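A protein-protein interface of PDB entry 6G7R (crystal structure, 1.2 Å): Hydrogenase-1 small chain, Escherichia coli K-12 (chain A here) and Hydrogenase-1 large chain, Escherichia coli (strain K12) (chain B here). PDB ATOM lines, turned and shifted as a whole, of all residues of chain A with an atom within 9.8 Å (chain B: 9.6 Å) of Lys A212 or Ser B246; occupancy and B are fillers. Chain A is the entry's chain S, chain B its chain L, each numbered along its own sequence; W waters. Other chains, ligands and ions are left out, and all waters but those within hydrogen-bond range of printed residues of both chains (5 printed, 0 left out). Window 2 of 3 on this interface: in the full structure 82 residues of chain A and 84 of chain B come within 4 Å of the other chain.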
ATOM      1  N   TYR A 191     -10.049 -28.277  -6.873  1.00  0.00           N
ATOM      2  CA  TYR A 191      -9.464 -26.930  -6.767  1.00  0.00           C
ATOM      3  C   TYR A 191      -8.087 -26.854  -7.410  1.00  0.00           C
ATOM      4  O   TYR A 191      -7.558 -25.753  -7.546  1.00  0.00           O
ATOM      5  CB  TYR A 191      -9.467 -26.438  -5.309  1.00  0.00           C
ATOM      6  CG  TYR A 191      -8.318 -26.927  -4.452  1.00  0.00           C
ATOM      7  CD1 TYR A 191      -7.979 -28.271  -4.310  1.00  0.00           C
ATOM      8  CD2 TYR A 191      -7.540 -26.019  -3.762  1.00  0.00           C
ATOM      9  CE1 TYR A 191      -6.907 -28.687  -3.536  1.00  0.00           C
ATOM     10  CE2 TYR A 191      -6.464 -26.414  -2.993  1.00  0.00           C
ATOM     11  CZ  TYR A 191      -6.135 -27.750  -2.895  1.00  0.00           C
ATOM     12  OH  TYR A 191      -5.037 -28.159  -2.187  1.00  0.00           O
ATOM     13  N   ARG A 192      -7.470 -27.972  -7.854  1.00  0.00           N
ATOM     14  CA  ARG A 192      -6.194 -27.907  -8.572  1.00  0.00           C
ATOM     15  C   ARG A 192      -6.395 -27.964 -10.087  1.00  0.00           C
ATOM     16  O   ARG A 192      -5.389 -28.001 -10.824  1.00  0.00           O
ATOM     17  CB  ARG A 192      -5.224 -28.979  -8.089  1.00  0.00           C
ATOM     18  CG  ARG A 192      -4.899 -28.842  -6.608  1.00  0.00           C
ATOM     19  CD  ARG A 192      -3.809 -29.778  -6.131  1.00  0.00           C
ATOM     20  NE  ARG A 192      -3.578 -29.608  -4.705  1.00  0.00           N
ATOM     21  CZ  ARG A 192      -2.478 -29.932  -4.050  1.00  0.00           C
ATOM     22  NH1 ARG A 192      -1.438 -30.470  -4.678  1.00  0.00           N
ATOM     23  NH2 ARG A 192      -2.453 -29.768  -2.740  1.00  0.00           N
ATOM     24  N   ALA A 194      -7.047 -25.592 -12.177  1.00  0.00           N
ATOM     25  CA  ALA A 194      -6.319 -24.528 -12.835  1.00  0.00           C
ATOM     26  C   ALA A 194      -4.935 -25.011 -13.261  1.00  0.00           C
ATOM     27  O   ALA A 194      -4.429 -24.654 -14.339  1.00  0.00           O
ATOM     28  CB  ALA A 194      -6.197 -23.345 -11.899  1.00  0.00           C
ATOM     29  N   HIS A 195      -4.290 -25.751 -12.369  1.00  0.00           N
ATOM     30  CA  HIS A 195      -2.933 -26.233 -12.629  1.00  0.00           C
ATOM     31  C   HIS A 195      -2.951 -27.326 -13.701  1.00  0.00           C
ATOM     32  O   HIS A 195      -2.108 -27.323 -14.596  1.00  0.00           O
ATOM     33  CB  HIS A 195      -2.285 -26.702 -11.344  1.00  0.00           C
ATOM     34  CG  HIS A 195      -2.189 -25.610 -10.317  1.00  0.00           C
ATOM     35  ND1 HIS A 195      -1.526 -24.429 -10.562  1.00  0.00           N
ATOM     36  CD2 HIS A 195      -2.669 -25.519  -9.052  1.00  0.00           C
ATOM     37  CE1 HIS A 195      -1.629 -23.674  -9.469  1.00  0.00           C
ATOM     38  NE2 HIS A 195      -2.295 -24.323  -8.523  1.00  0.00           N
ATOM     39  N   GLU A 200       0.701 -27.568 -15.096  1.00  0.00           N
ATOM     40  CA  GLU A 200       1.483 -27.294 -13.884  1.00  0.00           C
ATOM     41  C   GLU A 200       1.301 -28.476 -12.933  1.00  0.00           C
ATOM     42  O   GLU A 200       0.283 -28.599 -12.258  1.00  0.00           O
ATOM     43  CB  GLU A 200       0.999 -25.980 -13.249  1.00  0.00           C
ATOM     44  CG  GLU A 200       1.405 -24.765 -14.040  1.00  0.00           C
ATOM     45  CD  GLU A 200       0.772 -23.445 -13.659  1.00  0.00           C
ATOM     46  OE1 GLU A 200       1.234 -22.421 -14.206  1.00  0.00           O
ATOM     47  OE2 GLU A 200      -0.144 -23.440 -12.830  1.00  0.00           O
ATOM     48  N   PHE A 201       2.320 -29.351 -12.925  1.00  0.00           N
ATOM     49  CA  PHE A 201       2.223 -30.622 -12.248  1.00  0.00           C
ATOM     50  C   PHE A 201       3.350 -30.825 -11.236  1.00  0.00           C
ATOM     51  O   PHE A 201       4.500 -30.488 -11.484  1.00  0.00           O
ATOM     52  CB  PHE A 201       2.361 -31.739 -13.277  1.00  0.00           C
ATOM     53  CG  PHE A 201       1.299 -31.726 -14.334  1.00  0.00           C
ATOM     54  CD1 PHE A 201      -0.007 -31.972 -13.995  1.00  0.00           C
ATOM     55  CD2 PHE A 201       1.591 -31.476 -15.667  1.00  0.00           C
ATOM     56  CE1 PHE A 201      -1.006 -31.962 -14.954  1.00  0.00           C
ATOM     57  CE2 PHE A 201       0.593 -31.471 -16.620  1.00  0.00           C
ATOM     58  CZ  PHE A 201      -0.708 -31.734 -16.268  1.00  0.00           C
ATOM     59  N   VAL A 202       2.991 -31.463 -10.135  1.00  0.00           N
ATOM     60  CA  VAL A 202       3.998 -32.110  -9.278  1.00  0.00           C
ATOM     61  C   VAL A 202       4.694 -33.224 -10.053  1.00  0.00           C
ATOM     62  O   VAL A 202       4.039 -34.043 -10.674  1.00  0.00           O
ATOM     63  CB  VAL A 202       3.349 -32.673  -8.010  1.00  0.00           C
ATOM     64  CG1 VAL A 202       4.361 -33.369  -7.120  1.00  0.00           C
ATOM     65  CG2 VAL A 202       2.645 -31.566  -7.242  1.00  0.00           C
ATOM     66  N   GLN A 203       6.024 -33.217 -10.057  1.00  0.00           N
ATOM     67  CA  GLN A 203       6.783 -34.276 -10.746  1.00  0.00           C
ATOM     68  C   GLN A 203       7.455 -35.239  -9.791  1.00  0.00           C
ATOM     69  O   GLN A 203       7.702 -36.356 -10.207  1.00  0.00           O
ATOM     70  CB  GLN A 203       7.775 -33.655 -11.730  1.00  0.00           C
ATOM     71  CG  GLN A 203       7.065 -32.943 -12.869  1.00  0.00           C
ATOM     72  CD  GLN A 203       8.025 -32.258 -13.802  1.00  0.00           C
ATOM     73  OE1 GLN A 203       8.426 -31.116 -13.577  1.00  0.00           O
ATOM     74  NE2 GLN A 203       8.335 -32.941 -14.885  1.00  0.00           N
ATOM     75  N   SER A 204       7.803 -34.795  -8.617  1.00  0.00           N
ATOM     76  CA  SER A 204       8.317 -35.662  -7.568  1.00  0.00           C
ATOM     77  C   SER A 204       7.906 -35.079  -6.220  1.00  0.00           C
ATOM     78  O   SER A 204       7.677 -33.877  -6.116  1.00  0.00           O
ATOM     79  CB  SER A 204       9.798 -35.886  -7.662  1.00  0.00           C
ATOM     80  OG  SER A 204      10.492 -34.673  -7.580  1.00  0.00           O
ATOM     81  N   ASP A 206       7.424 -33.339  -2.826  1.00  0.00           N
ATOM     82  CA  ASP A 206       8.047 -32.235  -2.118  1.00  0.00           C
ATOM     83  C   ASP A 206       8.911 -31.366  -3.033  1.00  0.00           C
ATOM     84  O   ASP A 206       9.769 -30.627  -2.531  1.00  0.00           O
ATOM     85  CB  ASP A 206       8.818 -32.716  -0.888  1.00  0.00           C
ATOM     86  CG  ASP A 206       9.031 -31.626   0.155  1.00  0.00           C
ATOM     87  OD1 ASP A 206       8.182 -30.680   0.215  1.00  0.00           O
ATOM     88  OD2 ASP A 206       9.987 -31.764   0.943  1.00  0.00           O
ATOM     89  N   ASP A 207       8.643 -31.389  -4.335  1.00  0.00           N
ATOM     90  CA  ASP A 207       9.300 -30.471  -5.254  1.00  0.00           C
ATOM     91  C   ASP A 207       8.630 -29.087  -5.111  1.00  0.00           C
ATOM     92  O   ASP A 207       7.671 -28.855  -4.336  1.00  0.00           O
ATOM     93  CB  ASP A 207       9.322 -31.052  -6.677  1.00  0.00           C
ATOM     94  CG  ASP A 207       7.996 -31.172  -7.409  1.00  0.00           C
ATOM     95  OD1 ASP A 207       6.957 -30.781  -6.837  1.00  0.00           O
ATOM     96  OD2 ASP A 207       8.006 -31.705  -8.565  1.00  0.00           O
ATOM     97  N   ASP A 208       9.136 -28.099  -5.822  1.00  0.00           N
ATOM     98  CA  ASP A 208       8.607 -26.734  -5.695  1.00  0.00           C
ATOM     99  C   ASP A 208       7.128 -26.697  -6.093  1.00  0.00           C
ATOM    100  O   ASP A 208       6.327 -25.967  -5.462  1.00  0.00           O
ATOM    101  CB  ASP A 208       9.443 -25.753  -6.521  1.00  0.00           C
ATOM    102  CG  ASP A 208      10.816 -25.468  -5.915  1.00  0.00           C
ATOM    103  OD1 ASP A 208      11.122 -25.993  -4.807  1.00  0.00           O
ATOM    104  OD2 ASP A 208      11.577 -24.713  -6.544  1.00  0.00           O
ATOM    105  N   ALA A 209       6.754 -27.475  -7.095  1.00  0.00           N
ATOM    106  CA  ALA A 209       5.350 -27.590  -7.533  1.00  0.00           C
ATOM    107  C   ALA A 209       4.462 -28.107  -6.399  1.00  0.00           C
ATOM    108  O   ALA A 209       3.361 -27.601  -6.172  1.00  0.00           O
ATOM    109  CB  ALA A 209       5.275 -28.500  -8.745  1.00  0.00           C
ATOM    110  N   ALA A 210       4.939 -29.111  -5.690  1.00  0.00           N
ATOM    111  CA  ALA A 210       4.156 -29.679  -4.590  1.00  0.00           C
ATOM    112  C   ALA A 210       3.896 -28.636  -3.511  1.00  0.00           C
ATOM    113  O   ALA A 210       2.828 -28.581  -2.948  1.00  0.00           O
ATOM    114  CB  ALA A 210       4.840 -30.898  -3.990  1.00  0.00           C
ATOM    115  N   ARG A 211       4.901 -27.806  -3.254  1.00  0.00           N
ATOM    116  CA  ARG A 211       4.808 -26.787  -2.209  1.00  0.00           C
ATOM    117  C   ARG A 211       3.902 -25.615  -2.613  1.00  0.00           C
ATOM    118  O   ARG A 211       3.615 -24.779  -1.759  1.00  0.00           O
ATOM    119  CB  ARG A 211       6.206 -26.319  -1.819  1.00  0.00           C
ATOM    120  CG  ARG A 211       7.019 -27.368  -1.086  1.00  0.00           C
ATOM    121  CD  ARG A 211       8.464 -26.984  -0.858  1.00  0.00           C
ATOM    122  NE  ARG A 211       9.228 -28.041  -0.235  1.00  0.00           N
ATOM    123  CZ  ARG A 211      10.352 -27.861   0.433  1.00  0.00           C
ATOM    124  NH1 ARG A 211      10.911 -26.667   0.516  1.00  0.00           N
ATOM    125  NH2 ARG A 211      10.908 -28.905   1.024  1.00  0.00           N
ATOM    126  N   LYS A 212       3.484 -25.560  -3.881  1.00  0.00           N
ATOM    127  CA  LYS A 212       2.524 -24.588  -4.364  1.00  0.00           C
ATOM    128  C   LYS A 212       1.145 -25.179  -4.661  1.00  0.00           C
ATOM    129  O   LYS A 212       0.271 -24.474  -5.161  1.00  0.00           O
ATOM    130  CB  LYS A 212       3.056 -23.926  -5.647  1.00  0.00           C
ATOM    131  CG  LYS A 212       4.319 -23.110  -5.517  1.00  0.00           C
ATOM    132  CD  LYS A 212       4.758 -22.597  -6.857  1.00  0.00           C
ATOM    133  CE  LYS A 212       5.485 -23.576  -7.738  1.00  0.00           C
ATOM    134  NZ  LYS A 212       6.115 -22.892  -8.890  1.00  0.00           N
ATOM    135  N   GLY A 213       0.965 -26.458  -4.367  1.00  0.00           N
ATOM    136  CA  GLY A 213      -0.293 -27.126  -4.584  1.00  0.00           C
ATOM    137  C   GLY A 213      -0.614 -27.376  -6.049  1.00  0.00           C
ATOM    138  O   GLY A 213      -1.786 -27.343  -6.422  1.00  0.00           O
ATOM    139  N   TYR A 214       0.399 -27.713  -6.873  1.00  0.00           N
ATOM    140  CA  TYR A 214       0.128 -28.043  -8.269  1.00  0.00           C
ATOM    141  C   TYR A 214      -0.610 -29.381  -8.403  1.00  0.00           C
ATOM    142  O   TYR A 214      -0.741 -30.179  -7.450  1.00  0.00           O
ATOM    143  CB  TYR A 214       1.421 -28.007  -9.085  1.00  0.00           C
ATOM    144  CG  TYR A 214       1.945 -26.634  -9.439  1.00  0.00           C
ATOM    145  CD1 TYR A 214       1.397 -25.456  -8.951  1.00  0.00           C
ATOM    146  CD2 TYR A 214       2.994 -26.524 -10.337  1.00  0.00           C
ATOM    147  CE1 TYR A 214       1.919 -24.207  -9.282  1.00  0.00           C
ATOM    148  CE2 TYR A 214       3.481 -25.283 -10.729  1.00  0.00           C
ATOM    149  CZ  TYR A 214       2.968 -24.116 -10.182  1.00  0.00           C
ATOM    150  OH  TYR A 214       3.470 -22.903 -10.576  1.00  0.00           O
ATOM    151  N   CYS A 215      -1.103 -29.635  -9.620  1.00  0.00           N
ATOM    152  CA  CYS A 215      -1.911 -30.812  -9.903  1.00  0.00           C
ATOM    153  C   CYS A 215      -1.062 -32.078  -9.733  1.00  0.00           C
ATOM    154  O   CYS A 215       0.118 -32.117 -10.043  1.00  0.00           O
ATOM    155  CB  CYS A 215      -2.476 -30.695 -11.302  1.00  0.00           C
ATOM    156  SG  CYS A 215      -3.261 -32.172 -11.983  1.00  0.00           S
ATOM    157  N   LEU A 216      -1.753 -33.128  -9.287  1.00  0.00           N
ATOM    158  CA  LEU A 216      -1.178 -34.432  -8.946  1.00  0.00           C
ATOM    159  C   LEU A 216      -1.355 -35.482 -10.052  1.00  0.00           C
ATOM    160  O   LEU A 216      -1.046 -36.678  -9.828  1.00  0.00           O
ATOM    161  CB  LEU A 216      -1.766 -34.909  -7.606  1.00  0.00           C
ATOM    162  CG  LEU A 216      -1.442 -33.974  -6.456  1.00  0.00           C
ATOM    163  CD1 LEU A 216      -2.202 -34.337  -5.216  1.00  0.00           C
ATOM    164  CD2 LEU A 216       0.039 -33.922  -6.185  1.00  0.00           C
ATOM    165  N   ILE A 243      -6.293 -35.067  -2.138  1.00  0.00           N
ATOM    166  CA  ILE A 243      -5.541 -34.177  -3.009  1.00  0.00           C
ATOM    167  C   ILE A 243      -5.109 -32.908  -2.265  1.00  0.00           C
ATOM    168  O   ILE A 243      -3.979 -32.437  -2.465  1.00  0.00           O
ATOM    169  CB  ILE A 243      -6.379 -33.889  -4.262  1.00  0.00           C
ATOM    170  CG1 ILE A 243      -6.440 -35.121  -5.168  1.00  0.00           C
ATOM    171  CG2 ILE A 243      -5.902 -32.651  -5.001  1.00  0.00           C
ATOM    172  CD1 ILE A 243      -7.742 -35.230  -5.938  1.00  0.00           C
ATOM    173  N   GLN A 244      -5.989 -32.344  -1.417  1.00  0.00           N
ATOM    174  CA  GLN A 244      -5.637 -31.111  -0.708  1.00  0.00           C
ATOM    175  C   GLN A 244      -4.412 -31.330   0.184  1.00  0.00           C
ATOM    176  O   GLN A 244      -3.608 -30.415   0.369  1.00  0.00           O
ATOM    177  CB  GLN A 244      -6.838 -30.635   0.100  1.00  0.00           C
ATOM    178  CG  GLN A 244      -6.646 -29.310   0.790  1.00  0.00           C
ATOM    179  CD  GLN A 244      -7.927 -28.864   1.457  1.00  0.00           C
ATOM    180  OE1 GLN A 244      -9.007 -28.874   0.858  1.00  0.00           O
ATOM    181  NE2 GLN A 244      -7.791 -28.383   2.668  1.00  0.00           N
ATOM    182  N   GLY A 246      -2.044 -33.454  -0.525  1.00  0.00           N
ATOM    183  CA  GLY A 246      -0.862 -33.699  -1.324  1.00  0.00           C
ATOM    184  C   GLY A 246      -0.747 -35.073  -1.974  1.00  0.00           C
ATOM    185  O   GLY A 246       0.277 -35.327  -2.635  1.00  0.00           O
ATOM    186  N   PRO B 238       3.247 -37.061   1.977  1.00  0.00           N
ATOM    187  CA  PRO B 238       2.933 -36.262   0.805  1.00  0.00           C
ATOM    188  C   PRO B 238       2.497 -34.826   1.114  1.00  0.00           C
ATOM    189  O   PRO B 238       2.321 -34.036   0.166  1.00  0.00           O
ATOM    190  CB  PRO B 238       1.841 -37.043   0.073  1.00  0.00           C
ATOM    191  CG  PRO B 238       1.205 -37.928   1.111  1.00  0.00           C
ATOM    192  CD  PRO B 238       2.188 -38.045   2.258  1.00  0.00           C
ATOM    193  N   CYS B 239       2.330 -34.496   2.396  1.00  0.00           N
ATOM    194  CA  CYS B 239       1.814 -33.205   2.815  1.00  0.00           C
ATOM    195  C   CYS B 239       2.942 -32.172   2.868  1.00  0.00           C
ATOM    196  O   CYS B 239       3.419 -31.756   3.937  1.00  0.00           O
ATOM    197  CB  CYS B 239       1.071 -33.367   4.133  1.00  0.00           C
ATOM    198  SG  CYS B 239       2.072 -34.151   5.410  1.00  0.00           S
ATOM    199  N   ALA B 240       3.299 -31.687   1.690  1.00  0.00           N
ATOM    200  CA  ALA B 240       4.333 -30.672   1.525  1.00  0.00           C
ATOM    201  C   ALA B 240       3.981 -29.433   2.359  1.00  0.00           C
ATOM    202  O   ALA B 240       2.799 -29.038   2.477  1.00  0.00           O
ATOM    203  CB  ALA B 240       4.473 -30.294   0.066  1.00  0.00           C
ATOM    204  N   ILE B 241       5.024 -28.804   2.899  1.00  0.00           N
ATOM    205  CA  ILE B 241       4.904 -27.670   3.788  1.00  0.00           C
ATOM    206  C   ILE B 241       5.375 -26.399   3.071  1.00  0.00           C
ATOM    207  O   ILE B 241       6.396 -26.388   2.383  1.00  0.00           O
ATOM    208  CB  ILE B 241       5.715 -27.899   5.070  1.00  0.00           C
ATOM    209  CG1 ILE B 241       5.205 -29.138   5.812  1.00  0.00           C
ATOM    210  CG2 ILE B 241       5.709 -26.637   5.959  1.00  0.00           C
ATOM    211  CD1 ILE B 241       6.091 -29.557   6.934  1.00  0.00           C
ATOM    212  N   ASN B 242       4.625 -25.334   3.262  1.00  0.00           N
ATOM    213  CA  ASN B 242       4.971 -24.004   2.768  1.00  0.00           C
ATOM    214  C   ASN B 242       4.372 -23.027   3.764  1.00  0.00           C
ATOM    215  O   ASN B 242       3.154 -22.916   3.870  1.00  0.00           O
ATOM    216  CB  ASN B 242       4.405 -23.804   1.368  1.00  0.00           C
ATOM    217  CG  ASN B 242       4.706 -22.440   0.792  1.00  0.00           C
ATOM    218  OD1 ASN B 242       5.227 -21.561   1.489  1.00  0.00           O
ATOM    219  ND2 ASN B 242       4.400 -22.272  -0.493  1.00  0.00           N
ATOM    220  N   ILE B 243       5.235 -22.331   4.499  1.00  0.00           N
ATOM    221  CA  ILE B 243       4.769 -21.370   5.513  1.00  0.00           C
ATOM    222  C   ILE B 243       4.772 -19.939   4.980  1.00  0.00           C
ATOM    223  O   ILE B 243       3.876 -19.162   5.310  1.00  0.00           O
ATOM    224  CB  ILE B 243       5.644 -21.443   6.783  1.00  0.00           C
ATOM    225  CG1 ILE B 243       5.765 -22.864   7.313  1.00  0.00           C
ATOM    226  CG2 ILE B 243       5.106 -20.485   7.833  1.00  0.00           C
ATOM    227  CD1 ILE B 243       4.421 -23.474   7.603  1.00  0.00           C
ATOM    228  N   ASP B 244       5.777 -19.540   4.231  1.00  0.00           N
ATOM    229  CA  ASP B 244       6.030 -18.109   4.003  1.00  0.00           C
ATOM    230  C   ASP B 244       6.301 -17.789   2.534  1.00  0.00           C
ATOM    231  O   ASP B 244       6.862 -16.724   2.277  1.00  0.00           O
ATOM    232  CB  ASP B 244       7.185 -17.609   4.883  1.00  0.00           C
ATOM    233  CG  ASP B 244       7.375 -16.103   4.971  1.00  0.00           C
ATOM    234  OD1 ASP B 244       6.360 -15.400   5.011  1.00  0.00           O
ATOM    235  OD2 ASP B 244       8.527 -15.620   5.003  1.00  0.00           O
ATOM    236  N   GLU B 245       5.937 -18.663   1.610  1.00  0.00           N
ATOM    237  CA  GLU B 245       6.173 -18.419   0.193  1.00  0.00           C
ATOM    238  C   GLU B 245       4.841 -18.394  -0.562  1.00  0.00           C
ATOM    239  O   GLU B 245       3.806 -18.885  -0.077  1.00  0.00           O
ATOM    240  CB  GLU B 245       7.084 -19.494  -0.393  1.00  0.00           C
ATOM    241  CG  GLU B 245       8.441 -19.544   0.283  1.00  0.00           C
ATOM    242  CD  GLU B 245       9.132 -20.856  -0.052  1.00  0.00           C
ATOM    243  OE1 GLU B 245       9.214 -21.785   0.828  1.00  0.00           O
ATOM    244  OE2 GLU B 245       9.506 -20.992  -1.220  1.00  0.00           O
ATOM    245  N   SER B 246       4.891 -17.840  -1.765  1.00  0.00           N
ATOM    246  CA  SER B 246       3.744 -17.867  -2.652  1.00  0.00           C
ATOM    247  C   SER B 246       3.233 -19.304  -2.792  1.00  0.00           C
ATOM    248  O   SER B 246       4.001 -20.273  -2.891  1.00  0.00           O
ATOM    249  CB  SER B 246       4.089 -17.271  -3.990  1.00  0.00           C
ATOM    250  OG  SER B 246       2.935 -17.183  -4.803  1.00  0.00           O
ATOM    251  N   GLY B 247       1.916 -19.441  -2.812  1.00  0.00           N
ATOM    252  CA  GLY B 247       1.310 -20.718  -2.995  1.00  0.00           C
ATOM    253  C   GLY B 247       1.151 -21.531  -1.722  1.00  0.00           C
ATOM    254  O   GLY B 247       0.766 -22.714  -1.798  1.00  0.00           O
ATOM    255  N   ALA B 248       1.373 -20.924  -0.559  1.00  0.00           N
ATOM    256  CA  ALA B 248       1.176 -21.649   0.695  1.00  0.00           C
ATOM    257  C   ALA B 248      -0.268 -22.118   0.857  1.00  0.00           C
ATOM    258  O   ALA B 248      -0.528 -23.071   1.609  1.00  0.00           O
ATOM    259  CB  ALA B 248       1.599 -20.826   1.882  1.00  0.00           C
ATOM    260  N   VAL B 249      -1.208 -21.479   0.175  1.00  0.00           N
ATOM    261  CA  VAL B 249      -2.588 -21.946   0.125  1.00  0.00           C
ATOM    262  C   VAL B 249      -2.706 -23.381  -0.388  1.00  0.00           C
ATOM    263  O   VAL B 249      -3.739 -23.996  -0.165  1.00  0.00           O
ATOM    264  CB  VAL B 249      -3.493 -21.018  -0.710  1.00  0.00           C
ATOM    265  CG1 VAL B 249      -3.645 -19.660  -0.026  1.00  0.00           C
ATOM    266  CG2 VAL B 249      -2.992 -20.887  -2.141  1.00  0.00           C
ATOM    267  N   GLY B 250      -1.705 -23.843  -1.112  1.00  0.00           N
ATOM    268  CA  GLY B 250      -1.683 -25.199  -1.679  1.00  0.00           C
ATOM    269  C   GLY B 250      -0.927 -26.201  -0.831  1.00  0.00           C
ATOM    270  O   GLY B 250      -0.626 -27.288  -1.365  1.00  0.00           O
ATOM    271  N   ALA B 251      -0.602 -25.912   0.434  1.00  0.00           N
ATOM    272  CA  ALA B 251       0.291 -26.756   1.213  1.00  0.00           C
ATOM    273  C   ALA B 251      -0.090 -26.680   2.695  1.00  0.00           C
ATOM    274  O   ALA B 251      -1.018 -25.954   3.090  1.00  0.00           O
ATOM    275  CB  ALA B 251       1.697 -26.296   0.980  1.00  0.00           C
ATOM    276  N   VAL B 252       0.658 -27.384   3.518  1.00  0.00           N
ATOM    277  CA  VAL B 252       0.524 -27.243   4.971  1.00  0.00           C
ATOM    278  C   VAL B 252       1.168 -25.907   5.348  1.00  0.00           C
ATOM    279  O   VAL B 252       2.378 -25.723   5.199  1.00  0.00           O
ATOM    280  CB  VAL B 252       1.176 -28.425   5.710  1.00  0.00           C
ATOM    281  CG1 VAL B 252       1.163 -28.184   7.213  1.00  0.00           C
ATOM    282  CG2 VAL B 252       0.505 -29.731   5.357  1.00  0.00           C
ATOM    283  N   ASN B 253       0.316 -25.007   5.784  1.00  0.00           N
ATOM    284  CA  ASN B 253       0.690 -23.609   6.054  1.00  0.00           C
ATOM    285  C   ASN B 253       0.349 -23.286   7.516  1.00  0.00           C
ATOM    286  O   ASN B 253      -0.040 -24.172   8.283  1.00  0.00           O
ATOM    287  CB  ASN B 253      -0.020 -22.704   5.053  1.00  0.00           C
ATOM    288  CG  ASN B 253      -1.523 -22.775   5.150  1.00  0.00           C
ATOM    289  OD1 ASN B 253      -2.088 -22.772   6.242  1.00  0.00           O
ATOM    290  ND2 ASN B 253      -2.183 -22.927   4.009  1.00  0.00           N
HETATM  291  O   HOH W   1       4.803 -33.695  -2.007  1.00  0.00           O
HETATM  292  O   HOH W   2      -4.573 -26.573  -0.127  1.00  0.00           O
HETATM  293  O   HOH W   3       2.217 -33.354  -2.834  1.00  0.00           O
HETATM  294  O   HOH W   4      -0.206 -29.969  -0.901  1.00  0.00           O
HETATM  295  O   HOH W   5       7.612 -30.006   2.687  1.00  0.00           O
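Ala B240 touches Asp A206.
O of Ala A210 touches CB of Ala B240, 3.8 Å away.
Ile B241 touches Arg A211 (O to CG, 3.7 Å).
Arg A211 touches Gly B247.
Arg A211 touches Ala B251.
Lys A212 touches Ser B246.
Lys A212 touches Gly B247.
Gly A246 touches Pro B238 (CA to O, 3.5 Å).
Of the 23 printed residues of chain A, 7 touch a printed residue of chain B.
Printed residues of chain A that touch a printed residue of chain B: Arg A192, Asp A206, Ala A210, Arg A211, Lys A212, Gly A213 and Gly A246.
Among the printed residues, no Asp or Glu carboxylate lies within 4 Å of a Lys or Arg side-chain nitrogen of the other chain.
Lys A212 touches just these residues of chain B: Ser B246 and Gly B247.
Of chain A, only Lys A212 (3.9 Å) comes within 4 Å of Ser B246.
No residue of chain B comes within 4 Å of Ala A209.
Gly A213 touches just one residue of chain B: Gly B250 (3.2 Å).
Of chain A, only Arg A211 and Lys A212 come within 4 Å of Gly B247.
Printed residues of chain A within 4 Å of Ala B251: Arg A211.
Printed residues of chain B within 4 Å of Arg A192: Gly B250.
Asp A208 touches none of the printed residues of chain B.
The nearest residue of chain A that does not touch Ser B246 is Arg A211 (4.7 Å).
The nearest printed residue of chain B that does not touch Arg A211 is Ala B240 (4.05 Å).
Water W5 bridges the side-chain carboxylate (OD1) of Asp A206 (2.6 Å) and the backbone NH (N) of Ile B241 (2.9 Å).
Water W2 lies within hydrogen-bond range of OH of Tyr A191 (2.6 Å) and O of Val B249 (2.7 Å).
Water W4 lies within hydrogen-bond range of O of Gly B250 and NH2 of Arg A192.
Water W1 lies within hydrogen-bond range of the backbone NH of Asp A206 (2.8 Å) and the backbone carbonyl oxygen of Pro B238 (3.3 Å).
Water W3 lies within hydrogen-bond range of O of Gly A246 (2.8 Å) and O of Pro B238 (3.1 Å).
NH2 of Arg A192 lies within hydrogen-bond range of O of Ile A243 (3.1 Å).
NH2 of Arg A192 lies within hydrogen-bond range of O of Gln A244 (3.4 Å).
The side-chain carboxylate (OD1) of Asp A206 is in salt-bridge range of the guanidinium group (NE) of Arg A211 (2.9 Å).
N of Ala A210 lies within hydrogen-bond range of OD1 of Asp A207 (2.9 Å).
NZ of Lys A212 is in hydrogen-bond range of OH of Tyr A214 (3.1 Å).
The side-chain amide nitrogen of Asn B242 is in hydrogen-bond range of the backbone carbonyl oxygen of Ser B246 (3.1 Å).
The guanidinium group of Arg A192 is in hydrogen-bond range of the backbone carbonyl oxygen of Gly B250, at 3.4 Å.
N of Gly A213 sits close to O of Gly B250.
The backbone carbonyl oxygen (O) of Arg A211 lies within hydrogen-bond range of the side-chain amide nitrogen (ND2) of Asn B242 (2.9 Å).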
